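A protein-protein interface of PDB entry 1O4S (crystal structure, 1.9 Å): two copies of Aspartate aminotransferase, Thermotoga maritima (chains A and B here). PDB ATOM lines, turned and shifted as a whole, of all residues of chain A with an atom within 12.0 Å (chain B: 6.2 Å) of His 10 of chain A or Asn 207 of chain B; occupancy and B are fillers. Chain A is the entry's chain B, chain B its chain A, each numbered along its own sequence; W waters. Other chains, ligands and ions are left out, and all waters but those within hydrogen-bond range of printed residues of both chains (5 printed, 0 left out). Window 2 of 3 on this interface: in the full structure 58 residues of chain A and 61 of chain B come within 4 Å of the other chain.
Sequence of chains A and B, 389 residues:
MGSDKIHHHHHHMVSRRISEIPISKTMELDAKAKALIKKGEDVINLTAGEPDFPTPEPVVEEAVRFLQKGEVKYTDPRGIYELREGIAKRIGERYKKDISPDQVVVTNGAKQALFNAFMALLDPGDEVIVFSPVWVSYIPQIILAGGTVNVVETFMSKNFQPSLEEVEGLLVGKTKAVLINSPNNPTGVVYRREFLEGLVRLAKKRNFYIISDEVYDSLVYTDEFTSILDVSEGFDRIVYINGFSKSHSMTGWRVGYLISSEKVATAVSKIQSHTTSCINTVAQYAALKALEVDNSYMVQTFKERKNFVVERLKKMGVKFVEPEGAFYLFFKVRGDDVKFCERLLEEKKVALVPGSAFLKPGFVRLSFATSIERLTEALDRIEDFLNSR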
ATOM      1  N   ILE A   6      29.807  -4.639  21.206  1.00  0.00           N
ATOM      2  CA  ILE A   6      29.231  -3.310  20.894  1.00  0.00           C
ATOM      3  C   ILE A   6      28.311  -3.457  19.673  1.00  0.00           C
ATOM      4  O   ILE A   6      28.770  -3.805  18.567  1.00  0.00           O
ATOM      5  CB  ILE A   6      30.356  -2.281  20.510  1.00  0.00           C
ATOM      6  CG1 ILE A   6      31.442  -2.186  21.589  1.00  0.00           C
ATOM      7  CG2 ILE A   6      29.774  -0.875  20.193  1.00  0.00           C
ATOM      8  CD1 ILE A   6      32.591  -1.260  21.175  1.00  0.00           C
ATOM      9  N   HIS A   7      27.023  -3.189  19.859  1.00  0.00           N
ATOM     10  CA  HIS A   7      26.063  -3.392  18.778  1.00  0.00           C
ATOM     11  C   HIS A   7      25.622  -2.052  18.286  1.00  0.00           C
ATOM     12  O   HIS A   7      25.282  -1.201  19.085  1.00  0.00           O
ATOM     13  CB  HIS A   7      24.863  -4.194  19.231  1.00  0.00           C
ATOM     14  CG  HIS A   7      25.224  -5.530  19.782  1.00  0.00           C
ATOM     15  ND1 HIS A   7      25.779  -6.526  18.998  1.00  0.00           N
ATOM     16  CD2 HIS A   7      25.121  -6.037  21.034  1.00  0.00           C
ATOM     17  CE1 HIS A   7      26.003  -7.592  19.750  1.00  0.00           C
ATOM     18  NE2 HIS A   7      25.603  -7.325  20.985  1.00  0.00           N
ATOM     19  N   HIS A   8      25.683  -1.920  16.957  1.00  0.00           N
ATOM     20  CA  HIS A   8      25.219  -0.769  16.208  1.00  0.00           C
ATOM     21  C   HIS A   8      24.045  -1.174  15.288  1.00  0.00           C
ATOM     22  O   HIS A   8      23.980  -2.304  14.810  1.00  0.00           O
ATOM     23  CB  HIS A   8      26.369  -0.213  15.371  1.00  0.00           C
ATOM     24  CG  HIS A   8      27.537   0.266  16.176  1.00  0.00           C
ATOM     25  ND1 HIS A   8      27.583   1.519  16.752  1.00  0.00           N
ATOM     26  CD2 HIS A   8      28.723  -0.326  16.468  1.00  0.00           C
ATOM     27  CE1 HIS A   8      28.740   1.673  17.371  1.00  0.00           C
ATOM     28  NE2 HIS A   8      29.450   0.569  17.215  1.00  0.00           N
ATOM     29  N   HIS A   9      23.144  -0.223  15.049  1.00  0.00           N
ATOM     30  CA  HIS A   9      21.906  -0.418  14.269  1.00  0.00           C
ATOM     31  C   HIS A   9      21.758   0.734  13.272  1.00  0.00           C
ATOM     32  O   HIS A   9      22.054   1.892  13.611  1.00  0.00           O
ATOM     33  CB  HIS A   9      20.701  -0.522  15.228  1.00  0.00           C
ATOM     34  CG  HIS A   9      21.014  -1.340  16.439  1.00  0.00           C
ATOM     35  ND1 HIS A   9      20.845  -2.706  16.472  1.00  0.00           N
ATOM     36  CD2 HIS A   9      21.623  -1.007  17.605  1.00  0.00           C
ATOM     37  CE1 HIS A   9      21.284  -3.173  17.628  1.00  0.00           C
ATOM     38  NE2 HIS A   9      21.770  -2.163  18.330  1.00  0.00           N
ATOM     39  N   HIS A  10      21.347   0.400  12.045  1.00  0.00           N
ATOM     40  CA  HIS A  10      21.290   1.342  10.899  1.00  0.00           C
ATOM     41  C   HIS A  10      19.875   1.469  10.357  1.00  0.00           C
ATOM     42  O   HIS A  10      19.182   0.461  10.191  1.00  0.00           O
ATOM     43  CB  HIS A  10      22.161   0.837   9.740  1.00  0.00           C
ATOM     44  CG  HIS A  10      23.445   0.218  10.181  1.00  0.00           C
ATOM     45  ND1 HIS A  10      24.622   0.931  10.267  1.00  0.00           N
ATOM     46  CD2 HIS A  10      23.734  -1.043  10.586  1.00  0.00           C
ATOM     47  CE1 HIS A  10      25.582   0.136  10.704  1.00  0.00           C
ATOM     48  NE2 HIS A  10      25.071  -1.067  10.906  1.00  0.00           N
ATOM     49  N   HIS A  11      19.465   2.697  10.054  1.00  0.00           N
ATOM     50  CA  HIS A  11      18.203   2.963   9.361  1.00  0.00           C
ATOM     51  C   HIS A  11      18.400   2.797   7.867  1.00  0.00           C
ATOM     52  O   HIS A  11      19.503   3.043   7.330  1.00  0.00           O
ATOM     53  CB  HIS A  11      17.714   4.389   9.609  1.00  0.00           C
ATOM     54  CG  HIS A  11      17.299   4.662  11.025  1.00  0.00           C
ATOM     55  ND1 HIS A  11      18.198   4.985  12.019  1.00  0.00           N
ATOM     56  CD2 HIS A  11      16.075   4.663  11.610  1.00  0.00           C
ATOM     57  CE1 HIS A  11      17.544   5.172  13.154  1.00  0.00           C
ATOM     58  NE2 HIS A  11      16.255   4.984  12.933  1.00  0.00           N
ATOM     59  N   HIS A  12      17.327   2.400   7.191  1.00  0.00           N
ATOM     60  CA  HIS A  12      17.340   2.260   5.748  1.00  0.00           C
ATOM     61  C   HIS A  12      16.184   3.096   5.196  1.00  0.00           C
ATOM     62  O   HIS A  12      15.056   2.636   5.061  1.00  0.00           O
ATOM     63  CB  HIS A  12      17.340   0.775   5.378  1.00  0.00           C
ATOM     64  CG  HIS A  12      18.520   0.037   5.941  1.00  0.00           C
ATOM     65  ND1 HIS A  12      19.786   0.139   5.403  1.00  0.00           N
ATOM     66  CD2 HIS A  12      18.641  -0.760   7.033  1.00  0.00           C
ATOM     67  CE1 HIS A  12      20.631  -0.581   6.126  1.00  0.00           C
ATOM     68  NE2 HIS A  12      19.961  -1.143   7.115  1.00  0.00           N
ATOM     69  N   MET A  13      16.524   4.358   4.931  1.00  0.00           N
ATOM     70  CA  MET A  13      15.589   5.441   4.619  1.00  0.00           C
ATOM     71  C   MET A  13      15.374   5.541   3.133  1.00  0.00           C
ATOM     72  O   MET A  13      16.320   5.406   2.355  1.00  0.00           O
ATOM     73  CB  MET A  13      16.151   6.791   5.082  1.00  0.00           C
ATOM     74  CG  MET A  13      16.592   6.843   6.561  1.00  0.00           C
ATOM     75  SD  MET A  13      15.204   6.721   7.746  1.00  0.00           S
ATOM     76  CE  MET A  13      14.699   4.987   7.684  1.00  0.00           C
ATOM     77  N   VAL A  14      14.129   5.779   2.752  1.00  0.00           N
ATOM     78  CA  VAL A  14      13.754   6.110   1.397  1.00  0.00           C
ATOM     79  C   VAL A  14      13.353   7.589   1.406  1.00  0.00           C
ATOM     80  O   VAL A  14      13.252   8.189   2.476  1.00  0.00           O
ATOM     81  CB  VAL A  14      12.628   5.175   0.888  1.00  0.00           C
ATOM     82  CG1 VAL A  14      13.015   3.711   1.080  1.00  0.00           C
ATOM     83  CG2 VAL A  14      11.299   5.474   1.563  1.00  0.00           C
ATOM     84  N   SER A  15      13.191   8.203   0.243  1.00  0.00           N
ATOM     85  CA  SER A  15      12.868   9.622   0.199  1.00  0.00           C
ATOM     86  C   SER A  15      11.514   9.915   0.854  1.00  0.00           C
ATOM     87  O   SER A  15      10.582   9.117   0.775  1.00  0.00           O
ATOM     88  CB  SER A  15      12.910  10.179  -1.213  1.00  0.00           C
ATOM     89  OG  SER A  15      11.815   9.813  -1.942  1.00  0.00           O
ATOM     90  N   GLY B 173      26.437  13.851   5.603  1.00  0.00           N
ATOM     91  CA  GLY B 173      25.181  13.229   6.006  1.00  0.00           C
ATOM     92  C   GLY B 173      24.132  13.122   4.919  1.00  0.00           C
ATOM     93  O   GLY B 173      23.393  12.170   4.917  1.00  0.00           O
ATOM     94  N   THR B 175      24.816  12.545   1.821  1.00  0.00           N
ATOM     95  CA  THR B 175      25.245  11.580   0.801  1.00  0.00           C
ATOM     96  C   THR B 175      24.358  10.333   0.873  1.00  0.00           C
ATOM     97  O   THR B 175      24.411   9.586   1.840  1.00  0.00           O
ATOM     98  CB  THR B 175      26.704  11.159   0.973  1.00  0.00           C
ATOM     99  OG1 THR B 175      27.597  12.279   0.908  1.00  0.00           O
ATOM    100  CG2 THR B 175      27.113  10.272  -0.190  1.00  0.00           C
ATOM    101  N   LYS B 176      23.529  10.130  -0.142  1.00  0.00           N
ATOM    102  CA  LYS B 176      22.536   9.064  -0.119  1.00  0.00           C
ATOM    103  C   LYS B 176      22.996   7.840  -0.927  1.00  0.00           C
ATOM    104  O   LYS B 176      22.565   6.691  -0.681  1.00  0.00           O
ATOM    105  CB  LYS B 176      21.174   9.625  -0.598  1.00  0.00           C
ATOM    106  CG  LYS B 176      19.936   8.747  -0.306  1.00  0.00           C
ATOM    107  CD  LYS B 176      19.507   8.598   1.197  1.00  0.00           C
ATOM    108  CE  LYS B 176      18.875   9.859   1.873  1.00  0.00           C
ATOM    109  NZ  LYS B 176      17.455  10.279   1.519  1.00  0.00           N
ATOM    110  N   LEU B 202      32.496   1.048   3.527  1.00  0.00           N
ATOM    111  CA  LEU B 202      32.270   2.463   3.649  1.00  0.00           C
ATOM    112  C   LEU B 202      30.769   2.776   3.679  1.00  0.00           C
ATOM    113  O   LEU B 202      30.351   3.694   4.374  1.00  0.00           O
ATOM    114  CB  LEU B 202      33.008   3.189   2.505  1.00  0.00           C
ATOM    115  CG  LEU B 202      33.195   4.704   2.526  1.00  0.00           C
ATOM    116  CD1 LEU B 202      33.908   5.173   3.844  1.00  0.00           C
ATOM    117  CD2 LEU B 202      33.943   5.158   1.257  1.00  0.00           C
ATOM    118  N   ALA B 203      29.968   2.002   2.934  1.00  0.00           N
ATOM    119  CA  ALA B 203      28.531   2.195   2.855  1.00  0.00           C
ATOM    120  C   ALA B 203      27.897   1.883   4.200  1.00  0.00           C
ATOM    121  O   ALA B 203      26.919   2.553   4.609  1.00  0.00           O
ATOM    122  CB  ALA B 203      27.914   1.315   1.765  1.00  0.00           C
ATOM    123  N   LYS B 204      28.430   0.876   4.883  1.00  0.00           N
ATOM    124  CA  LYS B 204      27.951   0.541   6.251  1.00  0.00           C
ATOM    125  C   LYS B 204      28.465   1.567   7.264  1.00  0.00           C
ATOM    126  O   LYS B 204      27.727   2.032   8.101  1.00  0.00           O
ATOM    127  CB  LYS B 204      28.382  -0.883   6.665  1.00  0.00           C
ATOM    128  CG  LYS B 204      27.957  -1.315   8.077  1.00  0.00           C
ATOM    129  CD  LYS B 204      27.689  -2.831   8.108  1.00  0.00           C
ATOM    130  CE  LYS B 204      27.215  -3.386   9.483  1.00  0.00           C
ATOM    131  NZ  LYS B 204      25.934  -4.234   9.306  1.00  0.00           N
ATOM    132  N   LYS B 205      29.722   1.951   7.160  1.00  0.00           N
ATOM    133  CA  LYS B 205      30.312   2.924   8.085  1.00  0.00           C
ATOM    134  C   LYS B 205      29.569   4.263   8.084  1.00  0.00           C
ATOM    135  O   LYS B 205      29.335   4.849   9.147  1.00  0.00           O
ATOM    136  CB  LYS B 205      31.766   3.169   7.700  1.00  0.00           C
ATOM    137  CG  LYS B 205      32.607   3.957   8.739  1.00  0.00           C
ATOM    138  CD  LYS B 205      33.859   4.609   8.090  1.00  0.00           C
ATOM    139  CE  LYS B 205      34.735   5.330   9.151  1.00  0.00           C
ATOM    140  NZ  LYS B 205      36.072   5.694   8.557  1.00  0.00           N
ATOM    141  N   ARG B 206      29.199   4.722   6.884  1.00  0.00           N
ATOM    142  CA  ARG B 206      28.712   6.087   6.665  1.00  0.00           C
ATOM    143  C   ARG B 206      27.290   6.179   6.135  1.00  0.00           C
ATOM    144  O   ARG B 206      26.818   7.272   5.801  1.00  0.00           O
ATOM    145  CB  ARG B 206      29.683   6.821   5.736  1.00  0.00           C
ATOM    146  CG  ARG B 206      30.963   7.179   6.456  1.00  0.00           C
ATOM    147  CD  ARG B 206      30.723   8.126   7.694  1.00  0.00           C
ATOM    148  NE  ARG B 206      31.593   9.223   7.418  1.00  0.00           N
ATOM    149  CZ  ARG B 206      31.273  10.460   7.130  1.00  0.00           C
ATOM    150  NH1 ARG B 206      30.066  10.955   7.226  1.00  0.00           N
ATOM    151  NH2 ARG B 206      32.259  11.238   6.846  1.00  0.00           N
ATOM    152  N   ASN B 207      26.618   5.022   6.047  1.00  0.00           N
ATOM    153  CA  ASN B 207      25.195   4.924   5.712  1.00  0.00           C
ATOM    154  C   ASN B 207      24.764   5.530   4.392  1.00  0.00           C
ATOM    155  O   ASN B 207      24.098   6.579   4.353  1.00  0.00           O
ATOM    156  CB  ASN B 207      24.369   5.588   6.815  1.00  0.00           C
ATOM    157  CG  ASN B 207      24.525   4.903   8.120  1.00  0.00           C
ATOM    158  OD1 ASN B 207      24.014   3.805   8.295  1.00  0.00           O
ATOM    159  ND2 ASN B 207      25.234   5.537   9.058  1.00  0.00           N
ATOM    160  N   PHE B 208      25.198   4.902   3.313  1.00  0.00           N
ATOM    161  CA  PHE B 208      24.681   5.189   2.006  1.00  0.00           C
ATOM    162  C   PHE B 208      24.434   3.901   1.229  1.00  0.00           C
ATOM    163  O   PHE B 208      24.929   2.839   1.567  1.00  0.00           O
ATOM    164  CB  PHE B 208      25.602   6.157   1.234  1.00  0.00           C
ATOM    165  CG  PHE B 208      27.026   5.683   1.079  1.00  0.00           C
ATOM    166  CD1 PHE B 208      27.380   4.791   0.074  1.00  0.00           C
ATOM    167  CD2 PHE B 208      28.018   6.143   1.925  1.00  0.00           C
ATOM    168  CE1 PHE B 208      28.697   4.388  -0.089  1.00  0.00           C
ATOM    169  CE2 PHE B 208      29.363   5.720   1.779  1.00  0.00           C
ATOM    170  CZ  PHE B 208      29.685   4.845   0.761  1.00  0.00           C
ATOM    171  N   TYR B 209      23.714   4.054   0.139  1.00  0.00           N
ATOM    172  CA  TYR B 209      23.409   2.982  -0.787  1.00  0.00           C
ATOM    173  C   TYR B 209      24.447   2.924  -1.865  1.00  0.00           C
ATOM    174  O   TYR B 209      24.936   3.951  -2.313  1.00  0.00           O
ATOM    175  CB  TYR B 209      22.052   3.227  -1.466  1.00  0.00           C
ATOM    176  CG  TYR B 209      20.859   3.113  -0.560  1.00  0.00           C
ATOM    177  CD1 TYR B 209      20.233   1.893  -0.340  1.00  0.00           C
ATOM    178  CD2 TYR B 209      20.343   4.228   0.071  1.00  0.00           C
ATOM    179  CE1 TYR B 209      19.117   1.782   0.498  1.00  0.00           C
ATOM    180  CE2 TYR B 209      19.218   4.132   0.922  1.00  0.00           C
ATOM    181  CZ  TYR B 209      18.610   2.893   1.118  1.00  0.00           C
ATOM    182  OH  TYR B 209      17.534   2.790   1.969  1.00  0.00           O
ATOM    183  N   ARG B 237      21.596  -2.066   1.739  1.00  0.00           N
ATOM    184  CA  ARG B 237      22.251  -0.876   1.178  1.00  0.00           C
ATOM    185  C   ARG B 237      22.622  -1.033  -0.308  1.00  0.00           C
ATOM    186  O   ARG B 237      23.442  -0.294  -0.813  1.00  0.00           O
ATOM    187  CB  ARG B 237      23.555  -0.565   1.935  1.00  0.00           C
ATOM    188  CG  ARG B 237      23.404  -0.093   3.348  1.00  0.00           C
ATOM    189  CD  ARG B 237      24.766   0.073   4.097  1.00  0.00           C
ATOM    190  NE  ARG B 237      24.564  -0.211   5.524  1.00  0.00           N
ATOM    191  CZ  ARG B 237      24.592  -1.437   6.081  1.00  0.00           C
ATOM    192  NH1 ARG B 237      24.864  -2.527   5.359  1.00  0.00           N
ATOM    193  NH2 ARG B 237      24.364  -1.572   7.385  1.00  0.00           N
HETATM  194  O   HOH W   1      14.966  10.175   3.386  1.00  0.00           O
HETATM  195  O   HOH W   2      15.717   1.078   2.581  1.00  0.00           O
HETATM  196  O   HOH W   3      16.452   7.849   1.743  1.00  0.00           O
HETATM  197  O   HOH W   4      25.765   3.294  10.550  1.00  0.00           O
HETATM  198  O   HOH W   5      21.393   4.803  10.279  1.00  0.00           O
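O of Met 13 of chain A is in hydrogen-bond range of OH of Tyr 209 of chain B.
O of Lys 176 of chain B is in hydrogen-bond range of N of Tyr 209 of chain B (3.0 Å).
Among the printed residues, merely in contact across the chains: His 10 of chain A with Lys 204 of chain B, His 10 of chain A with Asn 207 of chain B, His 10 of chain A with Arg 237 of chain B, His 12 of chain A with Tyr 209 of chain B and His 12 of chain A with Arg 237 of chain B.
Of the printed residues of chain B, His 10 of chain A touches Lys 204 (3.5 Å), Asn 207 (3.5 Å) and Arg 237 (3.3 Å).
Printed residues of chain A within 4 Å of Asn 207 of chain B: His 10 (3.5 Å).
Gly 173 of chain B touches none of the printed residues of chain A.
No residue of chain A comes within 4 Å of Thr 175 of chain B.
Printed residues of chain A within 4 Å of Lys 204 of chain B: His 10.
No residue of chain A comes within 4 Å of Phe 208 of chain B.
Of the printed residues of chain B, His 12 of chain A touches Tyr 209 and Arg 237.
Of the printed residues of chain A, Arg 237 of chain B touches His 10 (3.3 Å) and His 12 (3.96 Å).
The nearest printed residue of chain B that does not touch His 10 of chain A is Lys 205 of chain B (5.7 Å).
Of the 10 printed residues of chain A, 3 touch a printed residue of chain B.
Of the 12 printed residues of chain B, 4 touch a printed residue of chain A.
Hydrophobic or aromatic side chains of chain B within 4 Å of the printed part of chain A: Tyr 209.
Among the printed residues, no Asp or Glu carboxylate lies within 4 Å of a Lys or Arg side-chain nitrogen of the other chain.
No position is printed for both chains.
Of the 6 pairs that touch across the chains among the printed residues, none has its exchanged pair printed and touching as well.
Water W3 lies within hydrogen-bond range of O of Met 13 of chain A, NZ of Lys 176 of chain B and N of Val 14 of chain A.
Water W2 bridges OH of Tyr 209 of chain B and O of His 12 of chain A.
Water W4 lies within hydrogen-bond range of a ring nitrogen (ND1) of His 10 of chain A (2.6 Å), the side-chain amide nitrogen (ND2) of Asn 207 of chain B (2.7 Å) and the backbone carbonyl oxygen (O) of Lys 204 of chain B (3.4 Å).
Water W1 lies within hydrogen-bond range of O of Val 14 of chain A (2.8 Å) and NZ of Lys 176 of chain B (3.1 Å).
Water W5 bridges the backbone NH of His 11 of chain A (2.9 Å) and the side-chain amide oxygen of Asn 207 of chain B (3.4 Å).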
